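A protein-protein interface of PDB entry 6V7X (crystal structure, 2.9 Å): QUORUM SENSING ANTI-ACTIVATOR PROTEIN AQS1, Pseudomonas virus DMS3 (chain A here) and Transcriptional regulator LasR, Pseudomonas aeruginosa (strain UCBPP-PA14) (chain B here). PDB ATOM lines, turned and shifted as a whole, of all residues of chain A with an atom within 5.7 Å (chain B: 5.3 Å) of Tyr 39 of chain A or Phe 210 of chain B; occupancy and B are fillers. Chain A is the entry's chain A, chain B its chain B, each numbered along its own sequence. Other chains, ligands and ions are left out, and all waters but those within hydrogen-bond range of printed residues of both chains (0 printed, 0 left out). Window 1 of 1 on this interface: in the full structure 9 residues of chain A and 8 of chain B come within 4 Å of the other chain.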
ATOM      1  N   TRP A  20     -14.425   5.925  18.606  1.00  0.00           N
ATOM      2  CA  TRP A  20     -13.613   6.318  19.755  1.00  0.00           C
ATOM      3  C   TRP A  20     -13.410   5.152  20.712  1.00  0.00           C
ATOM      4  O   TRP A  20     -12.285   4.883  21.152  1.00  0.00           O
ATOM      5  CB  TRP A  20     -14.272   7.497  20.477  1.00  0.00           C
ATOM      6  CG  TRP A  20     -13.456   8.058  21.616  1.00  0.00           C
ATOM      7  CD1 TRP A  20     -13.284   7.507  22.855  1.00  0.00           C
ATOM      8  CD2 TRP A  20     -12.715   9.285  21.620  1.00  0.00           C
ATOM      9  NE1 TRP A  20     -12.474   8.305  23.620  1.00  0.00           N
ATOM     10  CE2 TRP A  20     -12.112   9.404  22.888  1.00  0.00           C
ATOM     11  CE3 TRP A  20     -12.498  10.289  20.673  1.00  0.00           C
ATOM     12  CZ2 TRP A  20     -11.307  10.491  23.234  1.00  0.00           C
ATOM     13  CZ3 TRP A  20     -11.699  11.369  21.019  1.00  0.00           C
ATOM     14  CH2 TRP A  20     -11.113  11.460  22.288  1.00  0.00           C
ATOM     15  N   VAL A  23     -11.065   2.333  19.217  1.00  0.00           N
ATOM     16  CA  VAL A  23      -9.668   2.702  19.432  1.00  0.00           C
ATOM     17  C   VAL A  23      -9.320   2.655  20.913  1.00  0.00           C
ATOM     18  O   VAL A  23      -8.163   2.414  21.278  1.00  0.00           O
ATOM     19  CB  VAL A  23      -9.364   4.093  18.834  1.00  0.00           C
ATOM     20  CG1 VAL A  23      -7.860   4.339  18.805  1.00  0.00           C
ATOM     21  CG2 VAL A  23      -9.944   4.227  17.434  1.00  0.00           C
ATOM     22  N   LYS A  24     -10.304   2.864  21.791  1.00  0.00           N
ATOM     23  CA  LYS A  24     -10.030   2.903  23.226  1.00  0.00           C
ATOM     24  C   LYS A  24      -9.569   1.543  23.748  1.00  0.00           C
ATOM     25  O   LYS A  24      -8.492   1.430  24.348  1.00  0.00           O
ATOM     26  CB  LYS A  24     -11.270   3.393  23.980  1.00  0.00           C
ATOM     27  CG  LYS A  24     -11.205   3.208  25.489  1.00  0.00           C
ATOM     28  CD  LYS A  24     -12.557   3.474  26.127  1.00  0.00           C
ATOM     29  CE  LYS A  24     -12.685   2.749  27.451  1.00  0.00           C
ATOM     30  NZ  LYS A  24     -14.101   2.679  27.895  1.00  0.00           N
ATOM     31  N   SER A  27      -6.530   0.341  22.217  1.00  0.00           N
ATOM     32  CA  SER A  27      -5.379   0.955  22.864  1.00  0.00           C
ATOM     33  C   SER A  27      -5.230   0.492  24.306  1.00  0.00           C
ATOM     34  O   SER A  27      -4.114   0.493  24.838  1.00  0.00           O
ATOM     35  CB  SER A  27      -5.484   2.482  22.806  1.00  0.00           C
ATOM     36  OG  SER A  27      -5.978   3.014  24.025  1.00  0.00           O
ATOM     37  N   GLU A  31      -0.739   0.140  23.297  1.00  0.00           N
ATOM     38  CA  GLU A  31      -0.761   1.175  22.269  1.00  0.00           C
ATOM     39  C   GLU A  31       0.062   0.768  21.059  1.00  0.00           C
ATOM     40  O   GLU A  31      -0.197   1.248  19.949  1.00  0.00           O
ATOM     41  CB  GLU A  31      -0.251   2.494  22.843  1.00  0.00           C
ATOM     42  CG  GLU A  31      -1.045   3.001  24.037  1.00  0.00           C
ATOM     43  CD  GLU A  31      -0.752   2.200  25.299  1.00  0.00           C
ATOM     44  OE1 GLU A  31      -1.438   1.178  25.535  1.00  0.00           O
ATOM     45  OE2 GLU A  31       0.199   2.556  26.026  1.00  0.00           O
ATOM     46  N   VAL A  34      -2.172  -0.179  17.831  1.00  0.00           N
ATOM     47  CA  VAL A  34      -3.063   0.708  17.090  1.00  0.00           C
ATOM     48  C   VAL A  34      -2.245   1.697  16.263  1.00  0.00           C
ATOM     49  O   VAL A  34      -1.255   2.261  16.744  1.00  0.00           O
ATOM     50  CB  VAL A  34      -4.018   1.436  18.058  1.00  0.00           C
ATOM     51  CG1 VAL A  34      -3.235   2.045  19.206  1.00  0.00           C
ATOM     52  CG2 VAL A  34      -4.846   2.492  17.334  1.00  0.00           C
ATOM     53  N   HIS A  35      -2.672   1.916  15.020  1.00  0.00           N
ATOM     54  CA  HIS A  35      -2.007   2.851  14.113  1.00  0.00           C
ATOM     55  C   HIS A  35      -2.087   4.260  14.693  1.00  0.00           C
ATOM     56  O   HIS A  35      -3.180   4.813  14.845  1.00  0.00           O
ATOM     57  CB  HIS A  35      -2.648   2.777  12.727  1.00  0.00           C
ATOM     58  CG  HIS A  35      -3.089   1.395  12.340  1.00  0.00           C
ATOM     59  ND1 HIS A  35      -4.105   0.725  12.991  1.00  0.00           N
ATOM     60  CD2 HIS A  35      -2.636   0.548  11.385  1.00  0.00           C
ATOM     61  CE1 HIS A  35      -4.262  -0.470  12.450  1.00  0.00           C
ATOM     62  NE2 HIS A  35      -3.384  -0.601  11.472  1.00  0.00           N
ATOM     63  N   ASN A  36      -0.923   4.836  15.026  1.00  0.00           N
ATOM     64  CA  ASN A  36      -0.853   6.111  15.740  1.00  0.00           C
ATOM     65  C   ASN A  36      -1.691   7.210  15.092  1.00  0.00           C
ATOM     66  O   ASN A  36      -2.038   8.187  15.766  1.00  0.00           O
ATOM     67  CB  ASN A  36       0.616   6.552  15.853  1.00  0.00           C
ATOM     68  CG  ASN A  36       0.799   7.802  16.708  1.00  0.00           C
ATOM     69  OD1 ASN A  36       1.235   7.725  17.858  1.00  0.00           O
ATOM     70  ND2 ASN A  36       0.490   8.961  16.135  1.00  0.00           N
ATOM     71  N   ARG A  37      -2.035   7.073  13.812  1.00  0.00           N
ATOM     72  CA  ARG A  37      -2.799   8.090  13.100  1.00  0.00           C
ATOM     73  C   ARG A  37      -4.309   7.918  13.227  1.00  0.00           C
ATOM     74  O   ARG A  37      -5.054   8.753  12.704  1.00  0.00           O
ATOM     75  CB  ARG A  37      -2.398   8.114  11.618  1.00  0.00           C
ATOM     76  CG  ARG A  37      -0.971   8.586  11.372  1.00  0.00           C
ATOM     77  CD  ARG A  37      -0.039   7.429  11.026  1.00  0.00           C
ATOM     78  NE  ARG A  37       1.365   7.824  11.095  1.00  0.00           N
ATOM     79  CZ  ARG A  37       2.241   7.308  11.950  1.00  0.00           C
ATOM     80  NH1 ARG A  37       3.501   7.726  11.948  1.00  0.00           N
ATOM     81  NH2 ARG A  37       1.859   6.368  12.804  1.00  0.00           N
ATOM     82  N   SER A  38      -4.781   6.876  13.917  1.00  0.00           N
ATOM     83  CA  SER A  38      -6.212   6.752  14.166  1.00  0.00           C
ATOM     84  C   SER A  38      -6.624   7.550  15.398  1.00  0.00           C
ATOM     85  O   SER A  38      -7.783   7.958  15.516  1.00  0.00           O
ATOM     86  CB  SER A  38      -6.591   5.281  14.324  1.00  0.00           C
ATOM     87  OG  SER A  38      -5.706   4.631  15.208  1.00  0.00           O
ATOM     88  N   TYR A  39      -5.695   7.754  16.333  1.00  0.00           N
ATOM     89  CA  TYR A  39      -5.915   8.653  17.464  1.00  0.00           C
ATOM     90  C   TYR A  39      -6.402  10.017  16.992  1.00  0.00           C
ATOM     91  O   TYR A  39      -7.449  10.508  17.428  1.00  0.00           O
ATOM     92  CB  TYR A  39      -4.617   8.808  18.263  1.00  0.00           C
ATOM     93  CG  TYR A  39      -4.214   7.622  19.099  1.00  0.00           C
ATOM     94  CD1 TYR A  39      -2.899   7.179  19.107  1.00  0.00           C
ATOM     95  CD2 TYR A  39      -5.132   6.970  19.910  1.00  0.00           C
ATOM     96  CE1 TYR A  39      -2.508   6.105  19.887  1.00  0.00           C
ATOM     97  CE2 TYR A  39      -4.750   5.895  20.694  1.00  0.00           C
ATOM     98  CZ  TYR A  39      -3.438   5.467  20.680  1.00  0.00           C
ATOM     99  OH  TYR A  39      -3.065   4.397  21.464  1.00  0.00           O
ATOM    100  N   ARG A  40      -5.618  10.655  16.116  1.00  0.00           N
ATOM    101  CA  ARG A  40      -6.015  11.936  15.541  1.00  0.00           C
ATOM    102  C   ARG A  40      -7.363  11.832  14.845  1.00  0.00           C
ATOM    103  O   ARG A  40      -8.192  12.741  14.938  1.00  0.00           O
ATOM    104  CB  ARG A  40      -4.949  12.426  14.557  1.00  0.00           C
ATOM    105  CG  ARG A  40      -3.515  12.271  15.049  1.00  0.00           C
ATOM    106  CD  ARG A  40      -2.576  13.274  14.381  1.00  0.00           C
ATOM    107  NE  ARG A  40      -1.465  13.650  15.256  1.00  0.00           N
ATOM    108  CZ  ARG A  40      -1.303  14.850  15.812  1.00  0.00           C
ATOM    109  NH1 ARG A  40      -2.176  15.826  15.590  1.00  0.00           N
ATOM    110  NH2 ARG A  40      -0.254  15.074  16.592  1.00  0.00           N
ATOM    111  N   ASP A  41      -7.604  10.715  14.157  1.00  0.00           N
ATOM    112  CA  ASP A  41      -8.869  10.546  13.450  1.00  0.00           C
ATOM    113  C   ASP A  41     -10.043  10.493  14.419  1.00  0.00           C
ATOM    114  O   ASP A  41     -11.083  11.120  14.179  1.00  0.00           O
ATOM    115  CB  ASP A  41      -8.816   9.293  12.584  1.00  0.00           C
ATOM    116  CG  ASP A  41      -8.241   9.571  11.214  1.00  0.00           C
ATOM    117  OD1 ASP A  41      -7.062   9.235  10.972  1.00  0.00           O
ATOM    118  OD2 ASP A  41      -8.967  10.153  10.383  1.00  0.00           O
ATOM    119  N   ALA A  42      -9.895   9.760  15.523  1.00  0.00           N
ATOM    120  CA  ALA A  42     -10.956   9.730  16.522  1.00  0.00           C
ATOM    121  C   ALA A  42     -11.213  11.116  17.089  1.00  0.00           C
ATOM    122  O   ALA A  42     -12.355  11.454  17.420  1.00  0.00           O
ATOM    123  CB  ALA A  42     -10.600   8.751  17.640  1.00  0.00           C
ATOM    124  N   LEU A  43     -10.168  11.940  17.181  1.00  0.00           N
ATOM    125  CA  LEU A  43     -10.298  13.269  17.766  1.00  0.00           C
ATOM    126  C   LEU A  43     -10.962  14.248  16.804  1.00  0.00           C
ATOM    127  O   LEU A  43     -11.936  14.915  17.167  1.00  0.00           O
ATOM    128  CB  LEU A  43      -8.924  13.779  18.198  1.00  0.00           C
ATOM    129  CG  LEU A  43      -8.598  13.588  19.681  1.00  0.00           C
ATOM    130  CD1 LEU A  43      -7.105  13.726  19.947  1.00  0.00           C
ATOM    131  CD2 LEU A  43      -9.382  14.572  20.523  1.00  0.00           C
ATOM    132  N   ASP A  44     -10.455  14.351  15.570  1.00  0.00           N
ATOM    133  CA  ASP A  44     -11.017  15.325  14.640  1.00  0.00           C
ATOM    134  C   ASP A  44     -12.418  14.933  14.191  1.00  0.00           C
ATOM    135  O   ASP A  44     -13.243  15.814  13.919  1.00  0.00           O
ATOM    136  CB  ASP A  44     -10.099  15.518  13.429  1.00  0.00           C
ATOM    137  CG  ASP A  44      -9.568  14.213  12.878  1.00  0.00           C
ATOM    138  OD1 ASP A  44     -10.369  13.274  12.681  1.00  0.00           O
ATOM    139  OD2 ASP A  44      -8.345  14.131  12.636  1.00  0.00           O
ATOM    140  N   GLU B 205       0.969  13.587  20.292  1.00  0.00           N
ATOM    141  CA  GLU B 205       0.180  14.558  21.045  1.00  0.00           C
ATOM    142  C   GLU B 205      -1.295  14.176  21.052  1.00  0.00           C
ATOM    143  O   GLU B 205      -1.994  14.381  22.051  1.00  0.00           O
ATOM    144  CB  GLU B 205       0.368  15.962  20.471  1.00  0.00           C
ATOM    145  CG  GLU B 205      -0.375  17.034  21.253  1.00  0.00           C
ATOM    146  CD  GLU B 205      -0.191  18.417  20.671  1.00  0.00           C
ATOM    147  OE1 GLU B 205       0.477  18.533  19.621  1.00  0.00           O
ATOM    148  OE2 GLU B 205      -0.721  19.386  21.261  1.00  0.00           O
ATOM    149  N   ALA B 206      -1.788  13.618  19.945  1.00  0.00           N
ATOM    150  CA  ALA B 206      -3.163  13.138  19.931  1.00  0.00           C
ATOM    151  C   ALA B 206      -3.338  11.924  20.833  1.00  0.00           C
ATOM    152  O   ALA B 206      -4.443  11.676  21.324  1.00  0.00           O
ATOM    153  CB  ALA B 206      -3.593  12.810  18.503  1.00  0.00           C
ATOM    154  N   ASN B 207      -2.260  11.167  21.069  1.00  0.00           N
ATOM    155  CA  ASN B 207      -2.339  10.012  21.958  1.00  0.00           C
ATOM    156  C   ASN B 207      -2.685  10.435  23.382  1.00  0.00           C
ATOM    157  O   ASN B 207      -3.427   9.735  24.081  1.00  0.00           O
ATOM    158  CB  ASN B 207      -1.017   9.239  21.929  1.00  0.00           C
ATOM    159  CG  ASN B 207      -1.158   7.804  22.408  1.00  0.00           C
ATOM    160  OD1 ASN B 207      -0.301   6.963  22.134  1.00  0.00           O
ATOM    161  ND2 ASN B 207      -2.240   7.514  23.120  1.00  0.00           N
ATOM    162  N   VAL B 208      -2.156  11.574  23.835  1.00  0.00           N
ATOM    163  CA  VAL B 208      -2.471  12.033  25.185  1.00  0.00           C
ATOM    164  C   VAL B 208      -3.793  12.792  25.202  1.00  0.00           C
ATOM    165  O   VAL B 208      -4.562  12.697  26.165  1.00  0.00           O
ATOM    166  CB  VAL B 208      -1.317  12.876  25.767  1.00  0.00           C
ATOM    167  CG1 VAL B 208       0.006  12.163  25.583  1.00  0.00           C
ATOM    168  CG2 VAL B 208      -1.264  14.265  25.145  1.00  0.00           C
ATOM    169  N   ASN B 209      -4.083  13.553  24.143  1.00  0.00           N
ATOM    170  CA  ASN B 209      -5.391  14.190  24.041  1.00  0.00           C
ATOM    171  C   ASN B 209      -6.494  13.141  24.012  1.00  0.00           C
ATOM    172  O   ASN B 209      -7.568  13.338  24.593  1.00  0.00           O
ATOM    173  CB  ASN B 209      -5.449  15.076  22.795  1.00  0.00           C
ATOM    174  CG  ASN B 209      -4.668  16.363  22.954  1.00  0.00           C
ATOM    175  OD1 ASN B 209      -4.446  16.830  24.070  1.00  0.00           O
ATOM    176  ND2 ASN B 209      -4.240  16.941  21.837  1.00  0.00           N
ATOM    177  N   PHE B 210      -6.233  12.009  23.352  1.00  0.00           N
ATOM    178  CA  PHE B 210      -7.179  10.898  23.357  1.00  0.00           C
ATOM    179  C   PHE B 210      -7.316  10.306  24.755  1.00  0.00           C
ATOM    180  O   PHE B 210      -8.431  10.057  25.227  1.00  0.00           O
ATOM    181  CB  PHE B 210      -6.732   9.829  22.357  1.00  0.00           C
ATOM    182  CG  PHE B 210      -7.600   8.608  22.350  1.00  0.00           C
ATOM    183  CD1 PHE B 210      -7.242   7.481  23.071  1.00  0.00           C
ATOM    184  CD2 PHE B 210      -8.777   8.589  21.626  1.00  0.00           C
ATOM    185  CE1 PHE B 210      -8.042   6.362  23.072  1.00  0.00           C
ATOM    186  CE2 PHE B 210      -9.582   7.472  21.621  1.00  0.00           C
ATOM    187  CZ  PHE B 210      -9.214   6.356  22.343  1.00  0.00           C
ATOM    188  N   HIS B 211      -6.186  10.067  25.425  1.00  0.00           N
ATOM    189  CA  HIS B 211      -6.215   9.497  26.767  1.00  0.00           C
ATOM    190  C   HIS B 211      -6.992  10.387  27.724  1.00  0.00           C
ATOM    191  O   HIS B 211      -7.900   9.925  28.423  1.00  0.00           O
ATOM    192  CB  HIS B 211      -4.790   9.288  27.277  1.00  0.00           C
ATOM    193  CG  HIS B 211      -4.218   7.952  26.935  1.00  0.00           C
ATOM    194  ND1 HIS B 211      -5.003   6.832  26.760  1.00  0.00           N
ATOM    195  CD2 HIS B 211      -2.941   7.553  26.730  1.00  0.00           C
ATOM    196  CE1 HIS B 211      -4.233   5.801  26.464  1.00  0.00           C
ATOM    197  NE2 HIS B 211      -2.978   6.212  26.439  1.00  0.00           N
ATOM    198  N   MET B 212      -6.651  11.676  27.763  1.00  0.00           N
ATOM    199  CA  MET B 212      -7.325  12.579  28.687  1.00  0.00           C
ATOM    200  C   MET B 212      -8.821  12.637  28.422  1.00  0.00           C
ATOM    201  O   MET B 212      -9.608  12.806  29.359  1.00  0.00           O
ATOM    202  CB  MET B 212      -6.709  13.972  28.607  1.00  0.00           C
ATOM    203  CG  MET B 212      -6.505  14.604  29.966  1.00  0.00           C
ATOM    204  SD  MET B 212      -4.901  14.142  30.633  1.00  0.00           S
ATOM    205  CE  MET B 212      -3.806  15.106  29.595  1.00  0.00           C
ATOM    206  N   GLY B 213      -9.234  12.487  27.161  1.00  0.00           N
ATOM    207  CA  GLY B 213     -10.655  12.394  26.867  1.00  0.00           C
ATOM    208  C   GLY B 213     -11.312  11.210  27.550  1.00  0.00           C
ATOM    209  O   GLY B 213     -12.466  11.289  27.976  1.00  0.00           O
ATOM    210  N   ASN B 214     -10.584  10.098  27.666  1.00  0.00           N
ATOM    211  CA  ASN B 214     -11.093   8.967  28.434  1.00  0.00           C
ATOM    212  C   ASN B 214     -11.020   9.242  29.932  1.00  0.00           C
ATOM    213  O   ASN B 214     -11.899   8.816  30.688  1.00  0.00           O
ATOM    214  CB  ASN B 214     -10.312   7.700  28.086  1.00  0.00           C
ATOM    215  CG  ASN B 214     -10.435   7.317  26.622  1.00  0.00           C
ATOM    216  OD1 ASN B 214     -11.530   7.299  26.058  1.00  0.00           O
ATOM    217  ND2 ASN B 214      -9.306   7.004  26.000  1.00  0.00           N
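Printed residues of chain A that touch a printed residue of chain B: Trp 20, Val 23, Lys 24, Tyr 39, Arg 40 and Leu 43.
Hydrophobic or aromatic side chains of chain A within 4 Å of the printed part of chain B: Trp 20, Tyr 39 and Leu 43.
Hydrophobic or aromatic side chains of chain B within 4 Å of the printed part of chain A: Ala 206 and Phe 210.
Printed residues of chain B within 4 Å of Val 23 of chain A: Phe 210 (3.97 Å).
Printed residues of chain B within 4 Å of Tyr 39 of chain A: Asn 207 and Phe 210.
Printed residues of chain A within 4 Å of Asn 207 of chain B: Tyr 39.
Phe 210 of chain B touches just these residues of chain A: Trp 20 (3.4 Å), Val 23 (3.97 Å), Lys 24 (3.7 Å), Tyr 39 (3.8 Å) and Leu 43 (3.9 Å).
The nearest residue of chain A that does not touch Phe 210 of chain B is Ser 27 of chain A (4.05 Å).
The nearest printed residue of chain A that does not touch Asn 214 of chain B is Ser 27 of chain A (5.6 Å).
The indole nitrogen of Trp 20 of chain A is in hydrogen-bond range of the side-chain amide oxygen of Asn 214 of chain B (2.8 Å).
Trp 20 of chain A touches Phe 210 of chain B.
C of Val 23 of chain A touches CZ of Phe 210 of chain B, 3.97 Å away.
Lys 24 of chain A touches Phe 210 of chain B.
Lys 24 of chain A touches Asn 214 of chain B.
Tyr 39 of chain A touches Asn 207 of chain B (CE1 to OD1, 3.3 Å).
Tyr 39 of chain A touches Phe 210 of chain B.
CG of Arg 40 of chain A touches CB of Ala 206 of chain B, at 3.5 Å.
Leu 43 of chain A touches Ala 206 of chain B (CD1 to O, 3.6 Å).
CD1 of Leu 43 of chain A touches CB of Asn 209 of chain B, 3.6 Å away.
Phe 210 of chain B touches Leu 43 of chain A (N to CD1, 3.9 Å).
The backbone carbonyl oxygen (O) of Lys 24 of chain A lies within hydrogen-bond range of the side-chain hydroxyl (OG) of Ser 27 of chain A (3.0 Å).
O of Arg 40 of chain A sits close to OD2 of Asp 44 of chain A, 2.7 Å away.
ND2 of Asn 209 of chain B lies within hydrogen-bond range of O of Glu 205 of chain B.
ND2 of Asn 214 of chain B lies close to O of Phe 210 of chain B, at 3.3 Å.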
